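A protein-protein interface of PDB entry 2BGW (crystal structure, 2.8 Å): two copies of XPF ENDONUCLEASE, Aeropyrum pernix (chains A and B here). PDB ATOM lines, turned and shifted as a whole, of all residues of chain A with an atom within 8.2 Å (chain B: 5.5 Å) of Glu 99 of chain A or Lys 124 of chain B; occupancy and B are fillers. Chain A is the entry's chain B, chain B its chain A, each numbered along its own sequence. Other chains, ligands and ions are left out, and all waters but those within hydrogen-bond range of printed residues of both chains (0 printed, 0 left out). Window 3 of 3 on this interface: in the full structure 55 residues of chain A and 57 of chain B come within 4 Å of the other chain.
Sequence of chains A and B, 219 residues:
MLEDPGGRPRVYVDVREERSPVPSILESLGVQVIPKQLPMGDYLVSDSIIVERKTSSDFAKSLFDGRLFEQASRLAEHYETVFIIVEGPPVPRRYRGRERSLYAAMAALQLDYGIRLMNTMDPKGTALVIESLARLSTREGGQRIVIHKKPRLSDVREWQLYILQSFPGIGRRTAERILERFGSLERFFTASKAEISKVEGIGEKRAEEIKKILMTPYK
Of chain B, only Lys 124 comes within 4 Å of Glu 99 of chain A.
Of chain A, only Glu 99 (3.3 Å) comes within 4 Å of Lys 124 of chain B.
Gly 125 of chain B touches just one residue of chain A: Tyr 103 (3.6 Å).
Printed residues of chain A within 4 Å of Leu 128 of chain B: Tyr 103 (3.9 Å).
Printed residues of chain A within 4 Å of Val 129 of chain B: Tyr 103 (3.4 Å).
The backbone NH (N) of Gly 97 of chain A sits at hydrogen-bond distance from the side-chain carboxylate (OE2) of Glu 99 of chain A, 3.2 Å away.
The side-chain carboxylate (OD2) of Asp 122 of chain B lies within hydrogen-bond range of the backbone NH (N) of Gly 125 of chain B (3.0 Å).
Among the printed residues, pairs that only touch across the chains: Tyr 103 of chain A with Gly 125 of chain B (3.6 Å), Tyr 103 of chain A with Leu 128 of chain B (3.9 Å) and Tyr 103 of chain A with Val 129 of chain B (3.4 Å).
Hydrophobic or aromatic side chains of chain A within 4 Å of the printed part of chain B: Tyr 103.
Along chain A the printed residues that touch a printed residue of chain B span positions 99 to 103.
Of the 10 printed residues of chain B, 4 touch a printed residue of chain A.
Hydrophobic or aromatic side chains of chain B that line the printed part of chain A: Leu 128 and Val 129.
Among the printed residues, 4 pairs touch across the chains.
Among the printed residues, Asp or Glu carboxylates within 4 Å of a Lys or Arg side-chain nitrogen of the other chain: Glu 99 of chain A with Lys 124 of chain B (3.3 Å).
The side-chain carboxylate (OE1) of Glu 99 of chain A is in salt-bridge range of the side-chain amino group (NZ) of Lys 124 of chain B (3.3 Å).
No position is printed for both chains.
Of the 4 pairs that touch across the chains among the printed residues, none has its exchanged pair printed and touching as well.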
ATOM      1  N   LEU A  63      12.363  15.898 -11.171  1.00  0.00           N
ATOM      2  CA  LEU A  63      12.374  14.454 -10.942  1.00  0.00           C
ATOM      3  C   LEU A  63      12.122  14.193  -9.465  1.00  0.00           C
ATOM      4  O   LEU A  63      11.205  13.469  -9.109  1.00  0.00           O
ATOM      5  CB  LEU A  63      13.671  13.770 -11.401  1.00  0.00           C
ATOM      6  CG  LEU A  63      13.859  12.284 -10.993  1.00  0.00           C
ATOM      7  CD1 LEU A  63      12.651  11.408 -11.340  1.00  0.00           C
ATOM      8  CD2 LEU A  63      15.103  11.651 -11.566  1.00  0.00           C
ATOM      9  N   PHE A  64      12.914  14.819  -8.608  1.00  0.00           N
ATOM     10  CA  PHE A  64      12.834  14.569  -7.184  1.00  0.00           C
ATOM     11  C   PHE A  64      11.635  15.233  -6.495  1.00  0.00           C
ATOM     12  O   PHE A  64      11.254  14.777  -5.427  1.00  0.00           O
ATOM     13  CB  PHE A  64      14.175  14.882  -6.505  1.00  0.00           C
ATOM     14  CG  PHE A  64      15.309  13.960  -6.931  1.00  0.00           C
ATOM     15  CD1 PHE A  64      16.112  14.262  -8.032  1.00  0.00           C
ATOM     16  CD2 PHE A  64      15.570  12.769  -6.243  1.00  0.00           C
ATOM     17  CE1 PHE A  64      17.156  13.400  -8.442  1.00  0.00           C
ATOM     18  CE2 PHE A  64      16.619  11.907  -6.648  1.00  0.00           C
ATOM     19  CZ  PHE A  64      17.405  12.233  -7.752  1.00  0.00           C
ATOM     20  N   PRO A  90      23.409  15.538 -18.557  1.00  0.00           N
ATOM     21  CA  PRO A  90      22.341  14.715 -17.983  1.00  0.00           C
ATOM     22  C   PRO A  90      22.434  14.629 -16.458  1.00  0.00           C
ATOM     23  O   PRO A  90      21.421  14.658 -15.769  1.00  0.00           O
ATOM     24  CB  PRO A  90      22.605  13.344 -18.602  1.00  0.00           C
ATOM     25  CG  PRO A  90      23.303  13.635 -19.832  1.00  0.00           C
ATOM     26  CD  PRO A  90      24.175  14.795 -19.567  1.00  0.00           C
ATOM     27  N   VAL A  91      23.651  14.518 -15.939  1.00  0.00           N
ATOM     28  CA  VAL A  91      23.856  14.445 -14.508  1.00  0.00           C
ATOM     29  C   VAL A  91      24.624  15.662 -14.015  1.00  0.00           C
ATOM     30  O   VAL A  91      25.858  15.648 -14.000  1.00  0.00           O
ATOM     31  CB  VAL A  91      24.579  13.147 -14.101  1.00  0.00           C
ATOM     32  CG1 VAL A  91      24.646  13.051 -12.590  1.00  0.00           C
ATOM     33  CG2 VAL A  91      23.846  11.931 -14.669  1.00  0.00           C
ATOM     34  N   PRO A  92      23.905  16.715 -13.594  1.00  0.00           N
ATOM     35  CA  PRO A  92      24.548  17.896 -13.041  1.00  0.00           C
ATOM     36  C   PRO A  92      25.348  17.499 -11.811  1.00  0.00           C
ATOM     37  O   PRO A  92      25.015  16.498 -11.179  1.00  0.00           O
ATOM     38  CB  PRO A  92      23.365  18.766 -12.600  1.00  0.00           C
ATOM     39  CG  PRO A  92      22.186  18.278 -13.346  1.00  0.00           C
ATOM     40  CD  PRO A  92      22.439  16.822 -13.581  1.00  0.00           C
ATOM     41  N   TYR A  95      24.048  16.235  -8.427  1.00  0.00           N
ATOM     42  CA  TYR A  95      23.331  14.972  -8.450  1.00  0.00           C
ATOM     43  C   TYR A  95      24.154  13.755  -8.805  1.00  0.00           C
ATOM     44  O   TYR A  95      23.635  12.649  -8.868  1.00  0.00           O
ATOM     45  CB  TYR A  95      22.159  15.071  -9.394  1.00  0.00           C
ATOM     46  CG  TYR A  95      21.132  16.091  -9.008  1.00  0.00           C
ATOM     47  CD1 TYR A  95      21.173  17.368  -9.547  1.00  0.00           C
ATOM     48  CD2 TYR A  95      20.095  15.771  -8.136  1.00  0.00           C
ATOM     49  CE1 TYR A  95      20.228  18.316  -9.217  1.00  0.00           C
ATOM     50  CE2 TYR A  95      19.134  16.705  -7.804  1.00  0.00           C
ATOM     51  CZ  TYR A  95      19.206  17.981  -8.349  1.00  0.00           C
ATOM     52  OH  TYR A  95      18.261  18.937  -8.043  1.00  0.00           O
ATOM     53  N   ARG A  96      25.439  13.959  -9.047  1.00  0.00           N
ATOM     54  CA  ARG A  96      26.411  12.868  -9.048  1.00  0.00           C
ATOM     55  C   ARG A  96      26.115  12.035  -7.807  1.00  0.00           C
ATOM     56  O   ARG A  96      26.144  12.558  -6.692  1.00  0.00           O
ATOM     57  CB  ARG A  96      27.831  13.453  -8.956  1.00  0.00           C
ATOM     58  CG  ARG A  96      28.195  14.401 -10.107  1.00  0.00           C
ATOM     59  CD  ARG A  96      29.447  15.247  -9.800  1.00  0.00           C
ATOM     60  NE  ARG A  96      29.672  16.259 -10.846  1.00  0.00           N
ATOM     61  CZ  ARG A  96      30.543  16.138 -11.851  1.00  0.00           C
ATOM     62  NH1 ARG A  96      31.309  15.055 -11.964  1.00  0.00           N
ATOM     63  NH2 ARG A  96      30.652  17.107 -12.750  1.00  0.00           N
ATOM     64  N   GLY A  97      25.795  10.761  -7.965  1.00  0.00           N
ATOM     65  CA  GLY A  97      25.517   9.956  -6.770  1.00  0.00           C
ATOM     66  C   GLY A  97      24.047   9.625  -6.650  1.00  0.00           C
ATOM     67  O   GLY A  97      23.642   8.806  -5.830  1.00  0.00           O
ATOM     68  N   ARG A  98      23.246  10.272  -7.481  1.00  0.00           N
ATOM     69  CA  ARG A  98      21.890   9.838  -7.705  1.00  0.00           C
ATOM     70  C   ARG A  98      21.643   9.538  -9.185  1.00  0.00           C
ATOM     71  O   ARG A  98      20.507   9.562  -9.633  1.00  0.00           O
ATOM     72  CB  ARG A  98      20.927  10.899  -7.192  1.00  0.00           C
ATOM     73  CG  ARG A  98      20.858  10.936  -5.692  1.00  0.00           C
ATOM     74  CD  ARG A  98      21.094  12.310  -5.201  1.00  0.00           C
ATOM     75  NE  ARG A  98      19.855  13.033  -4.924  1.00  0.00           N
ATOM     76  CZ  ARG A  98      19.793  14.366  -4.796  1.00  0.00           C
ATOM     77  NH1 ARG A  98      20.887  15.130  -4.939  1.00  0.00           N
ATOM     78  NH2 ARG A  98      18.622  14.938  -4.536  1.00  0.00           N
ATOM     79  N   GLU A  99      22.688   9.234  -9.945  1.00  0.00           N
ATOM     80  CA  GLU A  99      22.490   9.025 -11.374  1.00  0.00           C
ATOM     81  C   GLU A  99      21.546   7.905 -11.689  1.00  0.00           C
ATOM     82  O   GLU A  99      20.826   7.986 -12.678  1.00  0.00           O
ATOM     83  CB  GLU A  99      23.771   8.695 -12.121  1.00  0.00           C
ATOM     84  CG  GLU A  99      24.921   9.455 -11.726  1.00  0.00           C
ATOM     85  CD  GLU A  99      25.933   8.506 -11.316  1.00  0.00           C
ATOM     86  OE1 GLU A  99      26.420   7.804 -12.233  1.00  0.00           O
ATOM     87  OE2 GLU A  99      26.172   8.413 -10.075  1.00  0.00           O
ATOM     88  N   ARG A 100      21.601   6.843 -10.887  1.00  0.00           N
ATOM     89  CA  ARG A 100      20.747   5.682 -11.095  1.00  0.00           C
ATOM     90  C   ARG A 100      19.312   6.167 -11.139  1.00  0.00           C
ATOM     91  O   ARG A 100      18.520   5.709 -11.951  1.00  0.00           O
ATOM     92  CB  ARG A 100      20.977   4.658  -9.986  1.00  0.00           C
ATOM     93  CG  ARG A 100      20.005   3.461  -9.966  1.00  0.00           C
ATOM     94  CD  ARG A 100      18.790   3.645  -8.972  1.00  0.00           C
ATOM     95  NE  ARG A 100      19.203   3.676  -7.553  1.00  0.00           N
ATOM     96  CZ  ARG A 100      18.405   4.043  -6.548  1.00  0.00           C
ATOM     97  NH1 ARG A 100      17.153   4.416  -6.787  1.00  0.00           N
ATOM     98  NH2 ARG A 100      18.862   4.052  -5.302  1.00  0.00           N
ATOM     99  N   SER A 101      19.002   7.133 -10.288  1.00  0.00           N
ATOM    100  CA  SER A 101      17.670   7.672 -10.225  1.00  0.00           C
ATOM    101  C   SER A 101      17.341   8.504 -11.434  1.00  0.00           C
ATOM    102  O   SER A 101      16.174   8.599 -11.837  1.00  0.00           O
ATOM    103  CB  SER A 101      17.482   8.500  -8.960  1.00  0.00           C
ATOM    104  OG  SER A 101      17.497   7.666  -7.810  1.00  0.00           O
ATOM    105  N   LEU A 102      18.360   9.124 -12.014  1.00  0.00           N
ATOM    106  CA  LEU A 102      18.129  10.013 -13.147  1.00  0.00           C
ATOM    107  C   LEU A 102      17.848   9.254 -14.442  1.00  0.00           C
ATOM    108  O   LEU A 102      16.851   9.494 -15.126  1.00  0.00           O
ATOM    109  CB  LEU A 102      19.280  11.012 -13.299  1.00  0.00           C
ATOM    110  CG  LEU A 102      19.106  12.273 -12.440  1.00  0.00           C
ATOM    111  CD1 LEU A 102      20.423  12.908 -12.169  1.00  0.00           C
ATOM    112  CD2 LEU A 102      18.173  13.271 -13.073  1.00  0.00           C
ATOM    113  N   TYR A 103      18.729   8.317 -14.753  1.00  0.00           N
ATOM    114  CA  TYR A 103      18.643   7.535 -15.955  1.00  0.00           C
ATOM    115  C   TYR A 103      17.413   6.664 -15.950  1.00  0.00           C
ATOM    116  O   TYR A 103      16.744   6.514 -16.980  1.00  0.00           O
ATOM    117  CB  TYR A 103      19.862   6.678 -16.051  1.00  0.00           C
ATOM    118  CG  TYR A 103      21.105   7.458 -16.366  1.00  0.00           C
ATOM    119  CD1 TYR A 103      22.180   7.479 -15.478  1.00  0.00           C
ATOM    120  CD2 TYR A 103      21.209   8.174 -17.547  1.00  0.00           C
ATOM    121  CE1 TYR A 103      23.334   8.173 -15.784  1.00  0.00           C
ATOM    122  CE2 TYR A 103      22.346   8.863 -17.856  1.00  0.00           C
ATOM    123  CZ  TYR A 103      23.413   8.871 -16.982  1.00  0.00           C
ATOM    124  OH  TYR A 103      24.560   9.584 -17.301  1.00  0.00           O
ATOM    125  N   ALA A 104      17.093   6.127 -14.779  1.00  0.00           N
ATOM    126  CA  ALA A 104      15.883   5.359 -14.616  1.00  0.00           C
ATOM    127  C   ALA A 104      14.650   6.185 -14.950  1.00  0.00           C
ATOM    128  O   ALA A 104      13.713   5.691 -15.527  1.00  0.00           O
ATOM    129  CB  ALA A 104      15.803   4.828 -13.212  1.00  0.00           C
ATOM    130  N   ALA A 105      14.653   7.450 -14.587  1.00  0.00           N
ATOM    131  CA  ALA A 105      13.549   8.322 -14.929  1.00  0.00           C
ATOM    132  C   ALA A 105      13.535   8.595 -16.406  1.00  0.00           C
ATOM    133  O   ALA A 105      12.483   8.862 -16.977  1.00  0.00           O
ATOM    134  CB  ALA A 105      13.650   9.625 -14.191  1.00  0.00           C
ATOM    135  N   MET A 106      14.704   8.562 -17.022  1.00  0.00           N
ATOM    136  CA  MET A 106      14.768   8.799 -18.450  1.00  0.00           C
ATOM    137  C   MET A 106      14.211   7.592 -19.178  1.00  0.00           C
ATOM    138  O   MET A 106      13.502   7.746 -20.182  1.00  0.00           O
ATOM    139  CB  MET A 106      16.193   9.055 -18.882  1.00  0.00           C
ATOM    140  CG  MET A 106      16.743  10.372 -18.421  1.00  0.00           C
ATOM    141  SD  MET A 106      18.491  10.411 -18.794  1.00  0.00           S
ATOM    142  CE  MET A 106      18.781  12.143 -18.427  1.00  0.00           C
ATOM    143  N   ILE B  25      29.867  -3.648 -16.028  1.00  0.00           N
ATOM    144  CA  ILE B  25      29.021  -2.772 -15.232  1.00  0.00           C
ATOM    145  C   ILE B  25      27.620  -3.359 -15.124  1.00  0.00           C
ATOM    146  O   ILE B  25      27.068  -3.438 -14.025  1.00  0.00           O
ATOM    147  CB  ILE B  25      29.001  -1.335 -15.757  1.00  0.00           C
ATOM    148  CG1 ILE B  25      30.421  -0.789 -15.839  1.00  0.00           C
ATOM    149  CG2 ILE B  25      28.210  -0.458 -14.812  1.00  0.00           C
ATOM    150  CD1 ILE B  25      30.517   0.536 -16.554  1.00  0.00           C
ATOM    151  N   GLU B  87      26.753   8.181 -25.797  1.00  0.00           N
ATOM    152  CA  GLU B  87      27.595   8.215 -24.621  1.00  0.00           C
ATOM    153  C   GLU B  87      28.660   9.319 -24.716  1.00  0.00           C
ATOM    154  O   GLU B  87      29.571   9.253 -25.575  1.00  0.00           O
ATOM    155  CB  GLU B  87      28.256   6.848 -24.478  1.00  0.00           C
ATOM    156  CG  GLU B  87      29.230   6.677 -23.338  1.00  0.00           C
ATOM    157  CD  GLU B  87      29.552   5.214 -23.138  1.00  0.00           C
ATOM    158  OE1 GLU B  87      28.611   4.456 -22.786  1.00  0.00           O
ATOM    159  OE2 GLU B  87      30.731   4.816 -23.348  1.00  0.00           O
ATOM    160  N   ASP B 122      28.832   8.441 -19.446  1.00  0.00           N
ATOM    161  CA  ASP B 122      29.923   7.500 -19.437  1.00  0.00           C
ATOM    162  C   ASP B 122      29.263   6.164 -19.588  1.00  0.00           C
ATOM    163  O   ASP B 122      28.042   6.102 -19.510  1.00  0.00           O
ATOM    164  CB  ASP B 122      30.660   7.555 -18.097  1.00  0.00           C
ATOM    165  CG  ASP B 122      29.749   7.908 -16.925  1.00  0.00           C
ATOM    166  OD1 ASP B 122      30.158   8.757 -16.117  1.00  0.00           O
ATOM    167  OD2 ASP B 122      28.630   7.359 -16.793  1.00  0.00           O
ATOM    168  N   PRO B 123      30.045   5.088 -19.807  1.00  0.00           N
ATOM    169  CA  PRO B 123      29.574   3.697 -19.774  1.00  0.00           C
ATOM    170  C   PRO B 123      28.578   3.346 -18.649  1.00  0.00           C
ATOM    171  O   PRO B 123      27.537   2.725 -18.910  1.00  0.00           O
ATOM    172  CB  PRO B 123      30.878   2.920 -19.580  1.00  0.00           C
ATOM    173  CG  PRO B 123      31.854   3.700 -20.374  1.00  0.00           C
ATOM    174  CD  PRO B 123      31.474   5.147 -20.158  1.00  0.00           C
ATOM    175  N   LYS B 124      28.904   3.734 -17.413  1.00  0.00           N
ATOM    176  CA  LYS B 124      28.049   3.462 -16.258  1.00  0.00           C
ATOM    177  C   LYS B 124      26.653   4.012 -16.500  1.00  0.00           C
ATOM    178  O   LYS B 124      25.671   3.410 -16.110  1.00  0.00           O
ATOM    179  CB  LYS B 124      28.654   4.089 -14.998  1.00  0.00           C
ATOM    180  CG  LYS B 124      28.009   3.664 -13.716  1.00  0.00           C
ATOM    181  CD  LYS B 124      28.077   4.748 -12.681  1.00  0.00           C
ATOM    182  CE  LYS B 124      27.693   4.212 -11.300  1.00  0.00           C
ATOM    183  NZ  LYS B 124      27.449   5.335 -10.330  1.00  0.00           N
ATOM    184  N   GLY B 125      26.576   5.158 -17.154  1.00  0.00           N
ATOM    185  CA  GLY B 125      25.293   5.740 -17.475  1.00  0.00           C
ATOM    186  C   GLY B 125      24.547   4.880 -18.480  1.00  0.00           C
ATOM    187  O   GLY B 125      23.343   4.643 -18.357  1.00  0.00           O
ATOM    188  N   THR B 126      25.270   4.412 -19.489  1.00  0.00           N
ATOM    189  CA  THR B 126      24.689   3.564 -20.528  1.00  0.00           C
ATOM    190  C   THR B 126      24.224   2.272 -19.886  1.00  0.00           C
ATOM    191  O   THR B 126      23.090   1.828 -20.126  1.00  0.00           O
ATOM    192  CB  THR B 126      25.700   3.292 -21.641  1.00  0.00           C
ATOM    193  OG1 THR B 126      26.286   4.546 -22.026  1.00  0.00           O
ATOM    194  CG2 THR B 126      25.035   2.647 -22.841  1.00  0.00           C
ATOM    195  N   ALA B 127      25.089   1.727 -19.026  1.00  0.00           N
ATOM    196  CA  ALA B 127      24.787   0.535 -18.257  1.00  0.00           C
ATOM    197  C   ALA B 127      23.556   0.716 -17.349  1.00  0.00           C
ATOM    198  O   ALA B 127      22.731  -0.194 -17.224  1.00  0.00           O
ATOM    199  CB  ALA B 127      25.963   0.126 -17.498  1.00  0.00           C
ATOM    200  N   LEU B 128      23.387   1.898 -16.777  1.00  0.00           N
ATOM    201  CA  LEU B 128      22.181   2.163 -16.015  1.00  0.00           C
ATOM    202  C   LEU B 128      20.930   2.235 -16.896  1.00  0.00           C
ATOM    203  O   LEU B 128      19.894   1.667 -16.561  1.00  0.00           O
ATOM    204  CB  LEU B 128      22.337   3.422 -15.160  1.00  0.00           C
ATOM    205  CG  LEU B 128      23.379   3.242 -14.050  1.00  0.00           C
ATOM    206  CD1 LEU B 128      23.985   4.566 -13.619  1.00  0.00           C
ATOM    207  CD2 LEU B 128      22.773   2.513 -12.868  1.00  0.00           C
ATOM    208  N   VAL B 129      21.032   2.920 -18.023  1.00  0.00           N
ATOM    209  CA  VAL B 129      19.894   3.115 -18.902  1.00  0.00           C
ATOM    210  C   VAL B 129      19.477   1.775 -19.472  1.00  0.00           C
ATOM    211  O   VAL B 129      18.286   1.464 -19.564  1.00  0.00           O
ATOM    212  CB  VAL B 129      20.263   4.095 -20.038  1.00  0.00           C
ATOM    213  CG1 VAL B 129      19.154   4.249 -21.048  1.00  0.00           C
ATOM    214  CG2 VAL B 129      20.569   5.423 -19.445  1.00  0.00           C
